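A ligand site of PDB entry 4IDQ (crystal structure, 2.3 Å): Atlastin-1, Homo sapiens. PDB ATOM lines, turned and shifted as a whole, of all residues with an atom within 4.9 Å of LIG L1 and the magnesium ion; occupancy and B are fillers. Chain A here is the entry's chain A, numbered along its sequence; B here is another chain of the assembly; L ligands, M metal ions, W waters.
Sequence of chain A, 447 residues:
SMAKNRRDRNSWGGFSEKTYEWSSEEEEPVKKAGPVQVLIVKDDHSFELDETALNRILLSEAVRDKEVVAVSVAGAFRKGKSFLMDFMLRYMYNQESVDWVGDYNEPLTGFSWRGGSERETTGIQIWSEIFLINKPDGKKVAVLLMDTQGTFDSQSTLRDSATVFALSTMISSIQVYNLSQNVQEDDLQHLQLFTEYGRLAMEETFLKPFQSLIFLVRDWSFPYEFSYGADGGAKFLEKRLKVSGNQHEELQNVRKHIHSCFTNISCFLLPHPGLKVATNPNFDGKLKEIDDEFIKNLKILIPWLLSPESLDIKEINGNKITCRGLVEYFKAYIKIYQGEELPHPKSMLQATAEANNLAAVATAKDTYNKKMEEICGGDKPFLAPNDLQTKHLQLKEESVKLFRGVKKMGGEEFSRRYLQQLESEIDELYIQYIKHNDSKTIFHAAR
Trp 113 touches LIG L1.
His 272 touches LIG L1.
Pro 273 touches LIG L1.
CD2 of Phe 283 touches O10 of LIG L1, at 3.8 Å.
CE2 of Phe 294 touches O11 of LIG L1, at 3.9 Å.
Of the 26 residues printed, 17 come within 4 Å of LIG L1.
AL1 of LG2 L2 is bound by O3 of LIG L1.
The magnesium ion is bound by an oxygen (O2) of LIG L1.
The magnesium ion is bound by a fluorine (F4) of LG2 L2.
Water W1 binds the magnesium ion, 2.0 Å away.
The side-chain hydroxyl (OG1) of Thr 121 is bound to the magnesium ion (2.1 Å).
The magnesium ion is bound by water W5 (2.2 Å).
The side-chain hydroxyl (OG) of Ser 82 is bound to the magnesium ion.
The magnesium ion has six donor atoms within binding distance.
OG of Ser 82 lies close to OD1 of Asp 147 (3.4 Å).
O of Ser 112 sits close to OG of Ser 82 (3.5 Å).
The side-chain amino group (NZ) of Lys 81 sits at hydrogen-bond distance from the backbone carbonyl oxygen (O) of Ala 76.
The backbone carbonyl oxygen (O) of Gly 80 sits at hydrogen-bond distance from the guanidinium group (NH1) of Arg 218, 3.0 Å away.
NH1 of Arg 78 lies within hydrogen-bond range of O of Arg 114, at 2.7 Å.
The backbone carbonyl oxygen (O) of Gly 115 sits at hydrogen-bond distance from the guanidinium group (NH1) of Arg 78 (3.5 Å).
The side-chain amino group of Lys 79 lies within hydrogen-bond range of the side-chain amide oxygen of Gln 181 of chain B.
Water W5 lies within hydrogen-bond range of OD1 of Asp 147 (2.6 Å) and O of Thr 148 (2.7 Å).
Water W1 bridges an oxygen (O6) of LIG L1 (2.8 Å) and the backbone carbonyl oxygen of Ser 112 (3.0 Å).
Water W4 lies within hydrogen-bond range of the backbone carbonyl oxygen (O) of Pro 271 (2.6 Å), an oxygen (O11) of LIG L1 (2.8 Å) and the backbone NH (N) of Asp 219 (2.9 Å).
Water W3 bridges a nitrogen (N4) of LIG L1 (2.9 Å) and the side-chain amide nitrogen (NE2) of Gln 181 of chain B (3.1 Å).
Water W6 lies within hydrogen-bond range of an oxygen (O8) of LIG L1 (2.9 Å) and the backbone carbonyl oxygen (O) of Arg 78 (2.9 Å).
Water W2 lies within hydrogen-bond range of the backbone carbonyl oxygen of Lys 79 (2.6 Å) and a nitrogen (N3) of LIG L1 (3.5 Å).
Asp 147 touches the magnesium ion (OD2 to MG, 3.8 Å).
Three residues have an atom within 4 Å of the magnesium ion: Ser 82, Thr 121 and Asp 147.
The nearest printed residue that does not touch the magnesium ion is Thr 148 (4.4 Å).
An oxygen (O5) of LIG L1 lies within hydrogen-bond range of the backbone NH (N) of Ser 82 (3.1 Å).
N of Lys 81 lies within hydrogen-bond range of O1 of LIG L1 (2.7 Å).
An oxygen (O1) of LIG L1 lies within salt-bridge range of the side-chain amino group of Lys 81 (2.6 Å).
OD1 of Asp 219 lies within hydrogen-bond range of N3 of LIG L1 (2.8 Å).
O5 of LIG L1 sits at hydrogen-bond distance from N of Phe 83.
The backbone NH (N) of Gly 80 lies within hydrogen-bond range of an oxygen (O4) of LIG L1.
An oxygen (O10) of LIG L1 is in hydrogen-bond range of the backbone carbonyl oxygen of Val 277 (2.9 Å).
The guanidinium group (NH2) of Arg 218 sits at hydrogen-bond distance from a nitrogen (N2) of LIG L1 (2.9 Å).
The backbone NH (N) of Arg 78 sits close to an oxygen (O3) of LIG L1 (3.2 Å).
The guanidinium group (NH2) of Arg 78 lies within salt-bridge range of an oxygen (O6) of LIG L1 (3.0 Å).
O1 of LIG L1 sits at hydrogen-bond distance from N of Lys 79, 3.1 Å away.
N of Arg 114 is in hydrogen-bond range of O6 of LIG L1, 3.2 Å away.
The backbone NH of Gly 115 sits close to an oxygen (O9) of LIG L1, 3.4 Å away.
The backbone NH (N) of Thr 121 is in hydrogen-bond range of a fluorine (F1) of LG2 L2 (3.0 Å).
The side-chain amino group (NZ) of Lys 81 sits at hydrogen-bond distance from a fluorine (F2) of LG2 L2, 2.5 Å away.
A fluorine (F3) of LG2 L2 lies within hydrogen-bond range of the backbone NH (N) of Arg 78, 2.7 Å away.
The guanidinium group of Arg 78 is in hydrogen-bond range of a fluorine (F1) of LG2 L2 (2.7 Å).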
ATOM      1  N   ALA A  76     -19.180   1.543  18.663  1.00  0.00           N
ATOM      2  CA  ALA A  76     -18.631   1.866  19.987  1.00  0.00           C
ATOM      3  C   ALA A  76     -17.370   2.747  19.899  1.00  0.00           C
ATOM      4  O   ALA A  76     -16.549   2.586  18.966  1.00  0.00           O
ATOM      5  CB  ALA A  76     -18.343   0.582  20.759  1.00  0.00           C
ATOM      6  N   PHE A  77     -17.200   3.652  20.870  1.00  0.00           N
ATOM      7  CA  PHE A  77     -16.029   4.543  20.884  1.00  0.00           C
ATOM      8  C   PHE A  77     -14.684   3.849  21.148  1.00  0.00           C
ATOM      9  O   PHE A  77     -14.622   2.750  21.702  1.00  0.00           O
ATOM     10  CB  PHE A  77     -16.253   5.779  21.800  1.00  0.00           C
ATOM     11  CG  PHE A  77     -15.899   5.555  23.246  1.00  0.00           C
ATOM     12  CD1 PHE A  77     -16.609   4.640  24.009  1.00  0.00           C
ATOM     13  CD2 PHE A  77     -14.884   6.290  23.849  1.00  0.00           C
ATOM     14  CE1 PHE A  77     -16.291   4.435  25.367  1.00  0.00           C
ATOM     15  CE2 PHE A  77     -14.557   6.090  25.197  1.00  0.00           C
ATOM     16  CZ  PHE A  77     -15.270   5.168  25.955  1.00  0.00           C
ATOM     17  N   ARG A  78     -13.616   4.504  20.707  1.00  0.00           N
ATOM     18  CA  ARG A  78     -12.235   4.014  20.855  1.00  0.00           C
ATOM     19  C   ARG A  78     -11.944   2.692  20.139  1.00  0.00           C
ATOM     20  O   ARG A  78     -11.151   1.909  20.628  1.00  0.00           O
ATOM     21  CB  ARG A  78     -11.859   3.853  22.327  1.00  0.00           C
ATOM     22  CG  ARG A  78     -12.042   5.062  23.220  1.00  0.00           C
ATOM     23  CD  ARG A  78     -10.977   6.136  23.037  1.00  0.00           C
ATOM     24  NE  ARG A  78     -11.051   6.813  21.754  1.00  0.00           N
ATOM     25  CZ  ARG A  78      -9.990   7.151  21.036  1.00  0.00           C
ATOM     26  NH1 ARG A  78      -8.785   6.855  21.492  1.00  0.00           N
ATOM     27  NH2 ARG A  78     -10.138   7.770  19.863  1.00  0.00           N
ATOM     28  N   LYS A  79     -12.563   2.442  18.981  1.00  0.00           N
ATOM     29  CA  LYS A  79     -12.325   1.167  18.304  1.00  0.00           C
ATOM     30  C   LYS A  79     -11.656   1.278  16.925  1.00  0.00           C
ATOM     31  O   LYS A  79     -11.690   0.321  16.142  1.00  0.00           O
ATOM     32  CB  LYS A  79     -13.618   0.342  18.192  1.00  0.00           C
ATOM     33  CG  LYS A  79     -14.339   0.126  19.512  1.00  0.00           C
ATOM     34  CD  LYS A  79     -13.512  -0.751  20.429  1.00  0.00           C
ATOM     35  CE  LYS A  79     -14.346  -1.354  21.546  1.00  0.00           C
ATOM     36  NZ  LYS A  79     -13.401  -1.877  22.586  1.00  0.00           N
ATOM     37  N   GLY A  80     -11.061   2.430  16.634  1.00  0.00           N
ATOM     38  CA  GLY A  80     -10.329   2.611  15.403  1.00  0.00           C
ATOM     39  C   GLY A  80     -11.195   2.973  14.200  1.00  0.00           C
ATOM     40  O   GLY A  80     -10.883   2.624  13.057  1.00  0.00           O
ATOM     41  N   LYS A  81     -12.312   3.628  14.458  1.00  0.00           N
ATOM     42  CA  LYS A  81     -13.138   4.102  13.347  1.00  0.00           C
ATOM     43  C   LYS A  81     -12.414   5.173  12.519  1.00  0.00           C
ATOM     44  O   LYS A  81     -12.355   5.075  11.291  1.00  0.00           O
ATOM     45  CB  LYS A  81     -14.515   4.597  13.841  1.00  0.00           C
ATOM     46  CG  LYS A  81     -15.379   3.513  14.494  1.00  0.00           C
ATOM     47  CD  LYS A  81     -16.745   4.051  14.946  1.00  0.00           C
ATOM     48  CE  LYS A  81     -16.638   5.222  15.944  1.00  0.00           C
ATOM     49  NZ  LYS A  81     -15.782   4.950  17.143  1.00  0.00           N
ATOM     50  N   SER A  82     -11.883   6.194  13.188  1.00  0.00           N
ATOM     51  CA  SER A  82     -11.229   7.295  12.477  1.00  0.00           C
ATOM     52  C   SER A  82      -9.992   6.809  11.733  1.00  0.00           C
ATOM     53  O   SER A  82      -9.686   7.246  10.619  1.00  0.00           O
ATOM     54  CB  SER A  82     -10.857   8.404  13.457  1.00  0.00           C
ATOM     55  OG  SER A  82     -12.010   9.062  13.965  1.00  0.00           O
ATOM     56  N   PHE A  83      -9.291   5.873  12.357  1.00  0.00           N
ATOM     57  CA  PHE A  83      -8.091   5.278  11.848  1.00  0.00           C
ATOM     58  C   PHE A  83      -8.424   4.569  10.510  1.00  0.00           C
ATOM     59  O   PHE A  83      -7.806   4.829   9.477  1.00  0.00           O
ATOM     60  CB  PHE A  83      -7.577   4.309  12.930  1.00  0.00           C
ATOM     61  CG  PHE A  83      -6.392   3.461  12.537  1.00  0.00           C
ATOM     62  CD1 PHE A  83      -5.101   3.895  12.792  1.00  0.00           C
ATOM     63  CD2 PHE A  83      -6.589   2.209  11.967  1.00  0.00           C
ATOM     64  CE1 PHE A  83      -4.017   3.099  12.457  1.00  0.00           C
ATOM     65  CE2 PHE A  83      -5.504   1.400  11.648  1.00  0.00           C
ATOM     66  CZ  PHE A  83      -4.223   1.849  11.890  1.00  0.00           C
ATOM     67  N   SER A 112      -8.952  13.012  12.801  1.00  0.00           N
ATOM     68  CA  SER A 112      -8.100  12.869  13.978  1.00  0.00           C
ATOM     69  C   SER A 112      -8.319  11.517  14.692  1.00  0.00           C
ATOM     70  O   SER A 112      -9.444  11.141  15.042  1.00  0.00           O
ATOM     71  CB  SER A 112      -8.304  14.062  14.937  1.00  0.00           C
ATOM     72  OG  SER A 112      -7.582  13.923  16.146  1.00  0.00           O
ATOM     73  N   TRP A 113      -7.235  10.778  14.886  1.00  0.00           N
ATOM     74  CA  TRP A 113      -7.275   9.480  15.537  1.00  0.00           C
ATOM     75  C   TRP A 113      -6.092   9.393  16.532  1.00  0.00           C
ATOM     76  O   TRP A 113      -5.061  10.026  16.321  1.00  0.00           O
ATOM     77  CB  TRP A 113      -7.199   8.345  14.512  1.00  0.00           C
ATOM     78  CG  TRP A 113      -5.842   8.214  13.853  1.00  0.00           C
ATOM     79  CD1 TRP A 113      -5.381   8.897  12.772  1.00  0.00           C
ATOM     80  CD2 TRP A 113      -4.752   7.363  14.280  1.00  0.00           C
ATOM     81  NE1 TRP A 113      -4.088   8.536  12.495  1.00  0.00           N
ATOM     82  CE2 TRP A 113      -3.682   7.598  13.398  1.00  0.00           C
ATOM     83  CE3 TRP A 113      -4.587   6.438  15.315  1.00  0.00           C
ATOM     84  CZ2 TRP A 113      -2.450   6.920  13.522  1.00  0.00           C
ATOM     85  CZ3 TRP A 113      -3.362   5.776  15.439  1.00  0.00           C
ATOM     86  CH2 TRP A 113      -2.314   6.015  14.548  1.00  0.00           C
ATOM     87  N   ARG A 114      -6.262   8.620  17.597  1.00  0.00           N
ATOM     88  CA  ARG A 114      -5.217   8.435  18.605  1.00  0.00           C
ATOM     89  C   ARG A 114      -5.603   7.361  19.619  1.00  0.00           C
ATOM     90  O   ARG A 114      -6.770   6.958  19.725  1.00  0.00           O
ATOM     91  CB  ARG A 114      -4.919   9.746  19.364  1.00  0.00           C
ATOM     92  CG  ARG A 114      -6.176  10.422  19.955  1.00  0.00           C
ATOM     93  CD  ARG A 114      -5.874  11.144  21.278  1.00  0.00           C
ATOM     94  NE  ARG A 114      -7.065  11.792  21.817  1.00  0.00           N
ATOM     95  CZ  ARG A 114      -7.948  11.210  22.653  1.00  0.00           C
ATOM     96  NH1 ARG A 114      -7.759   9.966  23.097  1.00  0.00           N
ATOM     97  NH2 ARG A 114      -8.999  11.899  23.068  1.00  0.00           N
ATOM     98  N   GLY A 115      -4.606   6.941  20.406  1.00  0.00           N
ATOM     99  CA  GLY A 115      -4.828   6.046  21.514  1.00  0.00           C
ATOM    100  C   GLY A 115      -5.317   6.851  22.715  1.00  0.00           C
ATOM    101  O   GLY A 115      -5.688   8.019  22.577  1.00  0.00           O
ATOM    102  N   THR A 121     -13.102  11.777  18.397  1.00  0.00           N
ATOM    103  CA  THR A 121     -14.111  12.278  17.469  1.00  0.00           C
ATOM    104  C   THR A 121     -15.430  12.583  18.195  1.00  0.00           C
ATOM    105  O   THR A 121     -15.929  11.717  18.902  1.00  0.00           O
ATOM    106  CB  THR A 121     -14.403  11.247  16.383  1.00  0.00           C
ATOM    107  OG1 THR A 121     -13.155  10.701  15.888  1.00  0.00           O
ATOM    108  CG2 THR A 121     -15.265  11.838  15.267  1.00  0.00           C
ATOM    109  N   ASP A 147     -17.113  10.679   9.371  1.00  0.00           N
ATOM    110  CA  ASP A 147     -16.566  10.061  10.575  1.00  0.00           C
ATOM    111  C   ASP A 147     -17.431  10.494  11.748  1.00  0.00           C
ATOM    112  O   ASP A 147     -17.889  11.640  11.802  1.00  0.00           O
ATOM    113  CB  ASP A 147     -15.099  10.455  10.767  1.00  0.00           C
ATOM    114  CG  ASP A 147     -14.396   9.617  11.837  1.00  0.00           C
ATOM    115  OD1 ASP A 147     -14.767   8.444  12.065  1.00  0.00           O
ATOM    116  OD2 ASP A 147     -13.437  10.131  12.440  1.00  0.00           O
ATOM    117  N   THR A 148     -17.698   9.587  12.678  1.00  0.00           N
ATOM    118  CA  THR A 148     -18.717   9.853  13.689  1.00  0.00           C
ATOM    119  C   THR A 148     -18.168   9.621  15.072  1.00  0.00           C
ATOM    120  O   THR A 148     -17.207   8.871  15.247  1.00  0.00           O
ATOM    121  CB  THR A 148     -20.002   9.003  13.504  1.00  0.00           C
ATOM    122  OG1 THR A 148     -19.768   7.653  13.937  1.00  0.00           O
ATOM    123  CG2 THR A 148     -20.450   8.998  12.039  1.00  0.00           C
ATOM    124  N   ARG A 218     -13.553  -6.000  14.081  1.00  0.00           N
ATOM    125  CA  ARG A 218     -12.143  -5.763  14.378  1.00  0.00           C
ATOM    126  C   ARG A 218     -11.635  -6.829  15.315  1.00  0.00           C
ATOM    127  O   ARG A 218     -12.373  -7.341  16.154  1.00  0.00           O
ATOM    128  CB  ARG A 218     -11.943  -4.375  14.996  1.00  0.00           C
ATOM    129  CG  ARG A 218     -12.631  -3.251  14.269  1.00  0.00           C
ATOM    130  CD  ARG A 218     -12.074  -2.972  12.862  1.00  0.00           C
ATOM    131  NE  ARG A 218     -10.886  -2.144  12.927  1.00  0.00           N
ATOM    132  CZ  ARG A 218     -10.861  -0.813  12.811  1.00  0.00           C
ATOM    133  NH1 ARG A 218     -11.977  -0.142  12.600  1.00  0.00           N
ATOM    134  NH2 ARG A 218      -9.707  -0.166  12.882  1.00  0.00           N
ATOM    135  N   ASP A 219     -10.356  -7.187  15.158  1.00  0.00           N
ATOM    136  CA  ASP A 219      -9.703  -8.121  16.071  1.00  0.00           C
ATOM    137  C   ASP A 219     -10.434  -9.456  16.160  1.00  0.00           C
ATOM    138  O   ASP A 219     -10.573 -10.025  17.225  1.00  0.00           O
ATOM    139  CB  ASP A 219      -9.567  -7.505  17.479  1.00  0.00           C
ATOM    140  CG  ASP A 219      -8.851  -6.165  17.460  1.00  0.00           C
ATOM    141  OD1 ASP A 219      -8.233  -5.837  16.444  1.00  0.00           O
ATOM    142  OD2 ASP A 219      -8.878  -5.457  18.479  1.00  0.00           O
ATOM    143  N   PRO A 271      -8.311  -9.079  10.923  1.00  0.00           N
ATOM    144  CA  PRO A 271      -7.435  -9.538  12.005  1.00  0.00           C
ATOM    145  C   PRO A 271      -6.981  -8.401  12.941  1.00  0.00           C
ATOM    146  O   PRO A 271      -7.080  -7.224  12.596  1.00  0.00           O
ATOM    147  CB  PRO A 271      -6.236 -10.176  11.266  1.00  0.00           C
ATOM    148  CG  PRO A 271      -6.308  -9.680   9.871  1.00  0.00           C
ATOM    149  CD  PRO A 271      -7.701  -9.234   9.583  1.00  0.00           C
ATOM    150  N   HIS A 272      -6.512  -8.770  14.134  1.00  0.00           N
ATOM    151  CA  HIS A 272      -5.862  -7.809  15.011  1.00  0.00           C
ATOM    152  C   HIS A 272      -4.670  -7.189  14.278  1.00  0.00           C
ATOM    153  O   HIS A 272      -3.893  -7.897  13.619  1.00  0.00           O
ATOM    154  CB  HIS A 272      -5.358  -8.509  16.304  1.00  0.00           C
ATOM    155  CG  HIS A 272      -5.130  -7.587  17.457  1.00  0.00           C
ATOM    156  ND1 HIS A 272      -4.120  -6.642  17.493  1.00  0.00           N
ATOM    157  CD2 HIS A 272      -5.778  -7.485  18.649  1.00  0.00           C
ATOM    158  CE1 HIS A 272      -4.164  -5.995  18.644  1.00  0.00           C
ATOM    159  NE2 HIS A 272      -5.167  -6.478  19.358  1.00  0.00           N
ATOM    160  N   PRO A 273      -4.498  -5.864  14.388  1.00  0.00           N
ATOM    161  CA  PRO A 273      -3.391  -5.198  13.695  1.00  0.00           C
ATOM    162  C   PRO A 273      -2.048  -5.287  14.425  1.00  0.00           C
ATOM    163  O   PRO A 273      -1.053  -4.692  13.962  1.00  0.00           O
ATOM    164  CB  PRO A 273      -3.859  -3.735  13.635  1.00  0.00           C
ATOM    165  CG  PRO A 273      -4.779  -3.597  14.798  1.00  0.00           C
ATOM    166  CD  PRO A 273      -5.425  -4.917  15.054  1.00  0.00           C
ATOM    167  N   VAL A 277       0.241  -1.354  17.376  1.00  0.00           N
ATOM    168  CA  VAL A 277      -0.854  -0.483  16.993  1.00  0.00           C
ATOM    169  C   VAL A 277      -1.772  -0.158  18.194  1.00  0.00           C
ATOM    170  O   VAL A 277      -2.196   0.991  18.392  1.00  0.00           O
ATOM    171  CB  VAL A 277      -1.693  -1.112  15.850  1.00  0.00           C
ATOM    172  CG1 VAL A 277      -2.938  -0.284  15.551  1.00  0.00           C
ATOM    173  CG2 VAL A 277      -0.844  -1.282  14.597  1.00  0.00           C
ATOM    174  N   ALA A 278      -2.076  -1.192  18.967  1.00  0.00           N
ATOM    175  CA  ALA A 278      -2.965  -1.098  20.132  1.00  0.00           C
ATOM    176  C   ALA A 278      -2.388  -0.350  21.341  1.00  0.00           C
ATOM    177  O   ALA A 278      -3.124   0.368  22.032  1.00  0.00           O
ATOM    178  CB  ALA A 278      -3.437  -2.490  20.532  1.00  0.00           C
ATOM    179  N   PHE A 283       3.028   5.041  18.332  1.00  0.00           N
ATOM    180  CA  PHE A 283       2.511   4.612  17.036  1.00  0.00           C
ATOM    181  C   PHE A 283       1.810   5.738  16.297  1.00  0.00           C
ATOM    182  O   PHE A 283       0.936   6.417  16.843  1.00  0.00           O
ATOM    183  CB  PHE A 283       1.575   3.392  17.160  1.00  0.00           C
ATOM    184  CG  PHE A 283       0.893   3.029  15.858  1.00  0.00           C
ATOM    185  CD1 PHE A 283       1.656   2.558  14.785  1.00  0.00           C
ATOM    186  CD2 PHE A 283      -0.476   3.144  15.710  1.00  0.00           C
ATOM    187  CE1 PHE A 283       1.049   2.227  13.586  1.00  0.00           C
ATOM    188  CE2 PHE A 283      -1.105   2.804  14.517  1.00  0.00           C
ATOM    189  CZ  PHE A 283      -0.336   2.354  13.449  1.00  0.00           C
ATOM    190  N   PHE A 294      -3.025  -8.154   8.818  1.00  0.00           N
ATOM    191  CA  PHE A 294      -3.945  -7.035   8.872  1.00  0.00           C
ATOM    192  C   PHE A 294      -3.925  -6.227   7.579  1.00  0.00           C
ATOM    193  O   PHE A 294      -4.971  -5.884   7.029  1.00  0.00           O
ATOM    194  CB  PHE A 294      -3.627  -6.148  10.085  1.00  0.00           C
ATOM    195  CG  PHE A 294      -4.499  -4.925  10.186  1.00  0.00           C
ATOM    196  CD1 PHE A 294      -4.194  -3.757   9.499  1.00  0.00           C
ATOM    197  CD2 PHE A 294      -5.658  -4.949  10.959  1.00  0.00           C
ATOM    198  CE1 PHE A 294      -5.005  -2.640   9.613  1.00  0.00           C
ATOM    199  CE2 PHE A 294      -6.482  -3.831  11.062  1.00  0.00           C
ATOM    200  CZ  PHE A 294      -6.147  -2.683  10.384  1.00  0.00           C
ATOM    201  N   GLN B 181     -11.202  -4.504  27.301  1.00  0.00           N
ATOM    202  CA  GLN B 181     -10.573  -3.265  26.836  1.00  0.00           C
ATOM    203  C   GLN B 181     -10.944  -1.987  27.530  1.00  0.00           C
ATOM    204  O   GLN B 181     -10.086  -1.131  27.690  1.00  0.00           O
ATOM    205  CB  GLN B 181     -10.830  -3.062  25.331  1.00  0.00           C
ATOM    206  CG  GLN B 181     -10.161  -4.073  24.449  1.00  0.00           C
ATOM    207  CD  GLN B 181     -10.675  -4.000  23.024  1.00  0.00           C
ATOM    208  OE1 GLN B 181     -11.783  -4.442  22.746  1.00  0.00           O
ATOM    209  NE2 GLN B 181      -9.868  -3.459  22.130  1.00  0.00           N
ATOM    210  N   PHE B 222      -3.673   0.909  27.297  1.00  0.00           N
ATOM    211  CA  PHE B 222      -3.040   2.207  27.557  1.00  0.00           C
ATOM    212  C   PHE B 222      -2.281   2.308  28.888  1.00  0.00           C
ATOM    213  O   PHE B 222      -2.566   3.175  29.719  1.00  0.00           O
ATOM    214  CB  PHE B 222      -4.096   3.302  27.464  1.00  0.00           C
ATOM    215  CG  PHE B 222      -5.099   3.059  26.372  1.00  0.00           C
ATOM    216  CD1 PHE B 222      -4.723   3.140  25.039  1.00  0.00           C
ATOM    217  CD2 PHE B 222      -6.405   2.725  26.670  1.00  0.00           C
ATOM    218  CE1 PHE B 222      -5.634   2.893  24.034  1.00  0.00           C
ATOM    219  CE2 PHE B 222      -7.325   2.481  25.667  1.00  0.00           C
ATOM    220  CZ  PHE B 222      -6.933   2.574  24.343  1.00  0.00           C
HETATM  221  P1  LIG L   1     -12.261   5.821  17.141  1.00  0.00           P
HETATM  222  O1  LIG L   1     -13.184   4.664  16.849  1.00  0.00           O
HETATM  223  O2  LIG L   1     -12.369   6.816  16.007  1.00  0.00           O
HETATM  224  O3  LIG L   1     -12.634   6.494  18.439  1.00  0.00           O
HETATM  225  O4  LIG L   1     -10.788   5.216  17.361  1.00  0.00           O
HETATM  226  P2  LIG L   1      -9.465   5.806  16.677  1.00  0.00           P
HETATM  227  O5  LIG L   1      -9.594   5.710  15.182  1.00  0.00           O
HETATM  228  O6  LIG L   1      -9.141   7.205  17.132  1.00  0.00           O
HETATM  229  O7  LIG L   1      -8.379   4.734  17.193  1.00  0.00           O
HETATM  230  C1  LIG L   1      -8.301   4.365  18.563  1.00  0.00           C
HETATM  231  C2  LIG L   1      -7.143   3.388  18.791  1.00  0.00           C
HETATM  232  O8  LIG L   1      -7.385   2.151  18.144  1.00  0.00           O
HETATM  233  C3  LIG L   1      -5.785   3.855  18.253  1.00  0.00           C
HETATM  234  O9  LIG L   1      -4.822   3.686  19.302  1.00  0.00           O
HETATM  235  C4  LIG L   1      -5.465   2.907  17.118  1.00  0.00           C
HETATM  236  O10 LIG L   1      -4.066   2.665  16.938  1.00  0.00           O
HETATM  237  C5  LIG L   1      -6.154   1.656  17.614  1.00  0.00           C
HETATM  238  N1  LIG L   1      -6.608   0.772  16.537  1.00  0.00           N
HETATM  239  C6  LIG L   1      -6.883   1.072  15.257  1.00  0.00           C
HETATM  240  N2  LIG L   1      -7.334  -0.030  14.609  1.00  0.00           N
HETATM  241  C7  LIG L   1      -7.339  -1.043  15.510  1.00  0.00           C
HETATM  242  C8  LIG L   1      -7.726  -2.464  15.533  1.00  0.00           C
HETATM  243  O11 LIG L   1      -8.146  -2.999  14.497  1.00  0.00           O
HETATM  244  N3  LIG L   1      -7.611  -3.145  16.681  1.00  0.00           N
HETATM  245  C9  LIG L   1      -7.167  -2.566  17.817  1.00  0.00           C
HETATM  246  N4  LIG L   1      -7.086  -3.322  18.942  1.00  0.00           N
HETATM  247  N5  LIG L   1      -6.800  -1.261  17.880  1.00  0.00           N
HETATM  248  C10 LIG L   1      -6.871  -0.489  16.781  1.00  0.00           C
HETATM  249 AL1  LG2 L   2     -13.902   7.898  19.050  1.00  0.00          AL
HETATM  250  F1  LG2 L   2     -12.490   8.964  19.320  1.00  0.00           F
HETATM  251  F2  LG2 L   2     -15.280   6.805  18.729  1.00  0.00           F
HETATM  252  F3  LG2 L   2     -13.632   7.188  20.665  1.00  0.00           F
HETATM  253  F4  LG2 L   2     -14.131   8.576  17.419  1.00  0.00           F
HETATM  254 MG    MG M   1     -12.914   8.585  15.917  1.00  0.00          MG
HETATM  255  O   HOH W   1     -11.083   9.086  16.463  1.00  0.00           O
HETATM  256  O   HOH W   2     -10.544  -1.519  17.526  1.00  0.00           O
HETATM  257  O   HOH W   3      -6.914  -2.658  21.770  1.00  0.00           O
HETATM  258  O   HOH W   4      -8.887  -5.454  13.354  1.00  0.00           O
HETATM  259  O   HOH W   5     -14.645   8.265  14.647  1.00  0.00           O
HETATM  260  O   HOH W   6      -9.204   0.152  19.279  1.00  0.00           O
